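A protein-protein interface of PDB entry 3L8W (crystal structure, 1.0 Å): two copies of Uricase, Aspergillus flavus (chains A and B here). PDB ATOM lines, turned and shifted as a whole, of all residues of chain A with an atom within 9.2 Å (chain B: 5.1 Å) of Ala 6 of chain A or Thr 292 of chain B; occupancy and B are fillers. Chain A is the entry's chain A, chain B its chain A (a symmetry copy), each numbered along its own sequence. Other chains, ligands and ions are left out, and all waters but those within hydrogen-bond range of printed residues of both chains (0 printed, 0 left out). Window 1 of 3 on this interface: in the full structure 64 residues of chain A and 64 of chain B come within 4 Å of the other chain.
Of the printed residues of chain A, Thr 292 of chain B touches Val 4 (3.7 Å), Lys 5 (2.7 Å) and Ala 6 (2.9 Å).
Of the printed residues of chain A, Lys 290 of chain B touches Ala 7 (3.5 Å), Arg 8 (2.9 Å) and Tyr 47 (2.8 Å).
Printed residues of chain B within 4 Å of Lys 5 of chain A: Thr 292 (2.7 Å).
Of the printed residues of chain B, Ser 2 of chain A touches Val 293 and Gly 294.
Ile 43 of chain A touches none of the printed residues of chain B.
Tyr 9 of chain A touches none of the printed residues of chain B.
The nearest printed residue of chain A that does not touch Thr 292 of chain B is Ala 3 of chain A (4.2 Å).
The nearest printed residue of chain B that does not touch Arg 8 of chain A is Cys 291 of chain B (5.1 Å).
Among the printed residues, pairs that only touch across the chains: Ser 2 of chain A with Gly 294 of chain B (3.2 Å), Ala 3 of chain A with Val 293 of chain B (3.4 Å), Ala 6 of chain A with Cys 291 of chain B (3.5 Å), Ala 7 of chain A with Lys 290 of chain B (3.5 Å), Tyr 47 of chain A with Cys 291 of chain B (3.5 Å), Val 4 of chain A with Thr 292 of chain B (3.7 Å) and Ser 2 of chain A with Val 293 of chain B (3.8 Å).
N of Ala 3 of chain A lies within hydrogen-bond range of O of Gly 294 of chain B, at 2.9 Å.
The backbone NH of Lys 5 of chain A lies within hydrogen-bond range of the backbone carbonyl oxygen of Thr 292 of chain B (2.7 Å).
The backbone NH (N) of Thr 292 of chain B is in hydrogen-bond range of the backbone carbonyl oxygen (O) of Ala 6 of chain A, 2.9 Å away.
N of Lys 290 of chain B lies within hydrogen-bond range of O of Arg 8 of chain A (2.9 Å).
The side-chain hydroxyl (OH) of Tyr 47 of chain A sits at hydrogen-bond distance from the backbone carbonyl oxygen (O) of Lys 290 of chain B, at 2.8 Å.
NH2 of Arg 8 of chain A is in salt-bridge range of OE2 of Glu 40 of chain A (3.6 Å).
The backbone carbonyl oxygen (O) of Val 249 of chain B sits at hydrogen-bond distance from the backbone NH (N) of Val 293 of chain B, 2.8 Å away.
No position is printed for both chains.
Of the 15 printed residues of chain A, 8 touch a printed residue of chain B.
Hydrophobic or aromatic side chains of chain A within 4 Å of the printed part of chain B: Ala 7 and Tyr 47.
Hydrophobic or aromatic side chains of chain B that line the printed part of chain A: Val 293.
Among the printed residues, 12 pairs touch across the chains.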
ATOM      1  N   SER A   2       9.244 -30.739  34.504  1.00  0.00           N
ATOM      2  CA  SER A   2      10.639 -30.956  34.123  1.00  0.00           C
ATOM      3  C   SER A   2      11.224 -29.619  33.687  1.00  0.00           C
ATOM      4  O   SER A   2      10.488 -28.665  33.464  1.00  0.00           O
ATOM      5  CB  SER A   2      10.798 -32.014  33.043  1.00  0.00           C
ATOM      6  OG  SER A   2      10.084 -31.745  31.869  1.00  0.00           O
ATOM      7  N   ALA A   3      12.558 -29.600  33.623  1.00  0.00           N
ATOM      8  CA  ALA A   3      13.304 -28.415  33.302  1.00  0.00           C
ATOM      9  C   ALA A   3      14.672 -28.793  32.740  1.00  0.00           C
ATOM     10  O   ALA A   3      15.238 -29.890  33.004  1.00  0.00           O
ATOM     11  CB  ALA A   3      13.551 -27.533  34.519  1.00  0.00           C
ATOM     12  N   VAL A   4      15.189 -27.906  31.904  1.00  0.00           N
ATOM     13  CA  VAL A   4      16.541 -28.091  31.372  1.00  0.00           C
ATOM     14  C   VAL A   4      17.596 -27.817  32.452  1.00  0.00           C
ATOM     15  O   VAL A   4      17.664 -26.711  33.015  1.00  0.00           O
ATOM     16  CB  VAL A   4      16.785 -27.177  30.177  1.00  0.00           C
ATOM     17  CG1 VAL A   4      18.224 -27.294  29.669  1.00  0.00           C
ATOM     18  CG2 VAL A   4      15.737 -27.450  29.084  1.00  0.00           C
ATOM     19  N   LYS A   5      18.424 -28.810  32.741  1.00  0.00           N
ATOM     20  CA  LYS A   5      19.503 -28.683  33.728  1.00  0.00           C
ATOM     21  C   LYS A   5      20.846 -28.300  33.102  1.00  0.00           C
ATOM     22  O   LYS A   5      21.707 -27.675  33.737  1.00  0.00           O
ATOM     23  CB  LYS A   5      19.750 -30.004  34.464  1.00  0.00           C
ATOM     24  CG  LYS A   5      20.847 -30.007  35.508  1.00  0.00           C
ATOM     25  CD  LYS A   5      20.932 -31.373  36.178  1.00  0.00           C
ATOM     26  CE  LYS A   5      22.040 -31.491  37.192  1.00  0.00           C
ATOM     27  NZ  LYS A   5      22.006 -32.776  37.936  1.00  0.00           N
ATOM     28  N   ALA A   6      21.064 -28.735  31.852  1.00  0.00           N
ATOM     29  CA  ALA A   6      22.268 -28.400  31.117  1.00  0.00           C
ATOM     30  C   ALA A   6      21.898 -28.446  29.625  1.00  0.00           C
ATOM     31  O   ALA A   6      21.019 -29.224  29.241  1.00  0.00           O
ATOM     32  CB  ALA A   6      23.411 -29.357  31.390  1.00  0.00           C
ATOM     33  N   ALA A   7      22.580 -27.614  28.851  1.00  0.00           N
ATOM     34  CA  ALA A   7      22.370 -27.644  27.397  1.00  0.00           C
ATOM     35  C   ALA A   7      23.582 -27.011  26.752  1.00  0.00           C
ATOM     36  O   ALA A   7      24.152 -26.010  27.206  1.00  0.00           O
ATOM     37  CB  ALA A   7      21.092 -26.929  27.040  1.00  0.00           C
ATOM     38  N   ARG A   8      23.966 -27.603  25.607  1.00  0.00           N
ATOM     39  CA  ARG A   8      24.939 -26.964  24.722  1.00  0.00           C
ATOM     40  C   ARG A   8      24.677 -27.491  23.317  1.00  0.00           C
ATOM     41  O   ARG A   8      24.168 -28.589  23.143  1.00  0.00           O
ATOM     42  CB  ARG A   8      26.367 -27.189  25.150  1.00  0.00           C
ATOM     43  CG  ARG A   8      26.830 -28.602  25.173  1.00  0.00           C
ATOM     44  CD  ARG A   8      28.314 -28.731  25.616  1.00  0.00           C
ATOM     45  NE  ARG A   8      28.469 -28.385  27.001  1.00  0.00           N
ATOM     46  CZ  ARG A   8      29.629 -28.335  27.638  1.00  0.00           C
ATOM     47  NH1 ARG A   8      30.769 -28.637  27.021  1.00  0.00           N
ATOM     48  NH2 ARG A   8      29.680 -28.006  28.907  1.00  0.00           N
ATOM     49  N   TYR A   9      25.046 -26.703  22.329  1.00  0.00           N
ATOM     50  CA  TYR A   9      24.777 -27.111  20.939  1.00  0.00           C
ATOM     51  C   TYR A   9      25.782 -26.362  20.075  1.00  0.00           C
ATOM     52  O   TYR A   9      26.280 -25.271  20.378  1.00  0.00           O
ATOM     53  CB  TYR A   9      23.270 -26.880  20.572  1.00  0.00           C
ATOM     54  CG  TYR A   9      23.154 -25.436  20.148  1.00  0.00           C
ATOM     55  CD1 TYR A   9      23.228 -24.384  21.082  1.00  0.00           C
ATOM     56  CD2 TYR A   9      23.122 -25.086  18.799  1.00  0.00           C
ATOM     57  CE1 TYR A   9      23.179 -23.080  20.693  1.00  0.00           C
ATOM     58  CE2 TYR A   9      23.128 -23.798  18.394  1.00  0.00           C
ATOM     59  CZ  TYR A   9      23.135 -22.808  19.349  1.00  0.00           C
ATOM     60  OH  TYR A   9      23.187 -21.484  18.949  1.00  0.00           O
ATOM     61  N   LEU A  39      28.061 -24.035  22.108  1.00  0.00           N
ATOM     62  CA  LEU A  39      27.681 -22.859  22.873  1.00  0.00           C
ATOM     63  C   LEU A  39      26.709 -23.190  23.970  1.00  0.00           C
ATOM     64  O   LEU A  39      25.892 -24.090  23.863  1.00  0.00           O
ATOM     65  CB  LEU A  39      27.004 -21.834  21.932  1.00  0.00           C
ATOM     66  CG  LEU A  39      27.818 -21.435  20.689  1.00  0.00           C
ATOM     67  CD1 LEU A  39      27.040 -20.354  19.924  1.00  0.00           C
ATOM     68  CD2 LEU A  39      29.217 -20.983  21.042  1.00  0.00           C
ATOM     69  N   GLU A  40      26.796 -22.382  25.052  1.00  0.00           N
ATOM     70  CA  GLU A  40      25.892 -22.432  26.193  1.00  0.00           C
ATOM     71  C   GLU A  40      25.376 -21.007  26.458  1.00  0.00           C
ATOM     72  O   GLU A  40      26.117 -20.033  26.212  1.00  0.00           O
ATOM     73  CB  GLU A  40      26.544 -22.895  27.486  1.00  0.00           C
ATOM     74  CG  GLU A  40      27.074 -24.270  27.570  1.00  0.00           C
ATOM     75  CD  GLU A  40      27.482 -24.513  29.036  1.00  0.00           C
ATOM     76  OE1 GLU A  40      26.634 -24.554  29.975  1.00  0.00           O
ATOM     77  OE2 GLU A  40      28.699 -24.599  29.200  1.00  0.00           O
ATOM     78  N   GLY A  41      24.174 -20.929  27.034  1.00  0.00           N
ATOM     79  CA  GLY A  41      23.698 -19.603  27.487  1.00  0.00           C
ATOM     80  C   GLY A  41      22.208 -19.702  27.726  1.00  0.00           C
ATOM     81  O   GLY A  41      21.662 -20.724  28.152  1.00  0.00           O
ATOM     82  N   ILE A  43      19.471 -20.371  26.416  1.00  0.00           N
ATOM     83  CA  ILE A  43      18.944 -21.093  25.257  1.00  0.00           C
ATOM     84  C   ILE A  43      17.865 -22.088  25.618  1.00  0.00           C
ATOM     85  O   ILE A  43      17.350 -22.813  24.754  1.00  0.00           O
ATOM     86  CB  ILE A  43      20.095 -21.781  24.464  1.00  0.00           C
ATOM     87  CG1 ILE A  43      20.806 -22.853  25.285  1.00  0.00           C
ATOM     88  CG2 ILE A  43      21.045 -20.733  23.879  1.00  0.00           C
ATOM     89  CD1 ILE A  43      21.836 -23.632  24.481  1.00  0.00           C
ATOM     90  N   GLU A  44      17.483 -22.189  26.880  1.00  0.00           N
ATOM     91  CA  GLU A  44      16.564 -23.233  27.311  1.00  0.00           C
ATOM     92  C   GLU A  44      15.223 -23.190  26.581  1.00  0.00           C
ATOM     93  O   GLU A  44      14.599 -24.252  26.349  1.00  0.00           O
ATOM     94  CB  GLU A  44      16.364 -23.260  28.828  1.00  0.00           C
ATOM     95  CG  GLU A  44      15.605 -22.108  29.439  1.00  0.00           C
ATOM     96  CD  GLU A  44      15.951 -21.795  30.880  1.00  0.00           C
ATOM     97  OE1 GLU A  44      17.159 -21.827  31.210  1.00  0.00           O
ATOM     98  OE2 GLU A  44      15.055 -21.488  31.697  1.00  0.00           O
ATOM     99  N   TYR A  47      14.474 -25.454  23.641  1.00  0.00           N
ATOM    100  CA  TYR A  47      14.108 -26.815  24.014  1.00  0.00           C
ATOM    101  C   TYR A  47      12.682 -26.908  24.521  1.00  0.00           C
ATOM    102  O   TYR A  47      11.943 -27.840  24.201  1.00  0.00           O
ATOM    103  CB  TYR A  47      15.096 -27.327  25.067  1.00  0.00           C
ATOM    104  CG  TYR A  47      16.560 -27.418  24.634  1.00  0.00           C
ATOM    105  CD1 TYR A  47      17.405 -26.323  24.707  1.00  0.00           C
ATOM    106  CD2 TYR A  47      17.109 -28.603  24.143  1.00  0.00           C
ATOM    107  CE1 TYR A  47      18.741 -26.389  24.324  1.00  0.00           C
ATOM    108  CE2 TYR A  47      18.455 -28.689  23.780  1.00  0.00           C
ATOM    109  CZ  TYR A  47      19.289 -27.599  23.866  1.00  0.00           C
ATOM    110  OH  TYR A  47      20.606 -27.647  23.489  1.00  0.00           O
ATOM    111  N   THR A  48      12.272 -25.955  25.374  1.00  0.00           N
ATOM    112  CA  THR A  48      10.989 -26.132  26.071  1.00  0.00           C
ATOM    113  C   THR A  48       9.820 -25.468  25.381  1.00  0.00           C
ATOM    114  O   THR A  48       8.669 -25.900  25.676  1.00  0.00           O
ATOM    115  CB  THR A  48      11.077 -25.546  27.501  1.00  0.00           C
ATOM    116  OG1 THR A  48      11.396 -24.157  27.371  1.00  0.00           O
ATOM    117  CG2 THR A  48      12.192 -26.159  28.315  1.00  0.00           C
ATOM    118  N   THR B 248      17.621 -37.775  35.914  1.00  0.00           N
ATOM    119  CA  THR B 248      17.827 -36.952  34.708  1.00  0.00           C
ATOM    120  C   THR B 248      17.826 -37.865  33.471  1.00  0.00           C
ATOM    121  O   THR B 248      18.140 -39.055  33.551  1.00  0.00           O
ATOM    122  CB  THR B 248      19.103 -36.111  34.699  1.00  0.00           C
ATOM    123  OG1 THR B 248      20.240 -37.001  34.752  1.00  0.00           O
ATOM    124  CG2 THR B 248      19.183 -35.157  35.849  1.00  0.00           C
ATOM    125  N   VAL B 249      17.509 -37.250  32.366  1.00  0.00           N
ATOM    126  CA  VAL B 249      17.621 -37.851  31.027  1.00  0.00           C
ATOM    127  C   VAL B 249      18.457 -36.886  30.168  1.00  0.00           C
ATOM    128  O   VAL B 249      18.176 -35.693  30.138  1.00  0.00           O
ATOM    129  CB  VAL B 249      16.253 -38.115  30.393  1.00  0.00           C
ATOM    130  CG1 VAL B 249      16.411 -38.630  28.989  1.00  0.00           C
ATOM    131  CG2 VAL B 249      15.411 -39.085  31.253  1.00  0.00           C
ATOM    132  N   GLU B 250      19.475 -37.421  29.488  1.00  0.00           N
ATOM    133  CA  GLU B 250      20.362 -36.643  28.629  1.00  0.00           C
ATOM    134  C   GLU B 250      20.263 -37.193  27.220  1.00  0.00           C
ATOM    135  O   GLU B 250      20.293 -38.399  27.016  1.00  0.00           O
ATOM    136  CB  GLU B 250      21.812 -36.786  29.074  1.00  0.00           C
ATOM    137  CG  GLU B 250      22.806 -35.943  28.377  1.00  0.00           C
ATOM    138  CD  GLU B 250      24.213 -35.936  28.934  1.00  0.00           C
ATOM    139  OE1 GLU B 250      24.507 -36.770  29.840  1.00  0.00           O
ATOM    140  OE2 GLU B 250      24.986 -35.091  28.408  1.00  0.00           O
ATOM    141  N   LYS B 290      22.784 -31.045  22.451  1.00  0.00           N
ATOM    142  CA  LYS B 290      22.804 -31.773  23.715  1.00  0.00           C
ATOM    143  C   LYS B 290      21.857 -31.127  24.725  1.00  0.00           C
ATOM    144  O   LYS B 290      21.729 -29.887  24.779  1.00  0.00           O
ATOM    145  CB  LYS B 290      24.216 -31.802  24.319  1.00  0.00           C
ATOM    146  CG  LYS B 290      25.258 -32.450  23.396  1.00  0.00           C
ATOM    147  CD  LYS B 290      26.646 -32.438  24.003  1.00  0.00           C
ATOM    148  CE  LYS B 290      27.693 -33.110  23.166  1.00  0.00           C
ATOM    149  NZ  LYS B 290      27.818 -34.552  23.408  1.00  0.00           N
ATOM    150  N   CYS B 291      21.245 -31.951  25.566  1.00  0.00           N
ATOM    151  CA  CYS B 291      20.362 -31.463  26.647  1.00  0.00           C
ATOM    152  C   CYS B 291      20.426 -32.465  27.784  1.00  0.00           C
ATOM    153  O   CYS B 291      20.377 -33.654  27.518  1.00  0.00           O
ATOM    154  CB  CYS B 291      18.944 -31.301  26.136  1.00  0.00           C
ATOM    155  SG  CYS B 291      17.750 -30.364  27.131  1.00  0.00           S
ATOM    156  N   THR B 292      20.380 -32.007  29.021  1.00  0.00           N
ATOM    157  CA  THR B 292      20.119 -32.772  30.224  1.00  0.00           C
ATOM    158  C   THR B 292      18.856 -32.202  30.878  1.00  0.00           C
ATOM    159  O   THR B 292      18.844 -31.018  31.181  1.00  0.00           O
ATOM    160  CB  THR B 292      21.266 -32.731  31.235  1.00  0.00           C
ATOM    161  OG1 THR B 292      22.441 -33.200  30.537  1.00  0.00           O
ATOM    162  CG2 THR B 292      21.010 -33.647  32.420  1.00  0.00           C
ATOM    163  N   VAL B 293      17.871 -33.062  31.047  1.00  0.00           N
ATOM    164  CA  VAL B 293      16.565 -32.678  31.581  1.00  0.00           C
ATOM    165  C   VAL B 293      16.384 -33.353  32.942  1.00  0.00           C
ATOM    166  O   VAL B 293      16.661 -34.540  33.078  1.00  0.00           O
ATOM    167  CB  VAL B 293      15.421 -33.074  30.634  1.00  0.00           C
ATOM    168  CG1 VAL B 293      14.042 -32.650  31.161  1.00  0.00           C
ATOM    169  CG2 VAL B 293      15.623 -32.447  29.239  1.00  0.00           C
ATOM    170  N   GLY B 294      15.929 -32.563  33.931  1.00  0.00           N
ATOM    171  CA  GLY B 294      15.656 -33.067  35.285  1.00  0.00           C
ATOM    172  C   GLY B 294      14.275 -32.591  35.694  1.00  0.00           C
ATOM    173  O   GLY B 294      13.518 -32.011  34.930  1.00  0.00           O
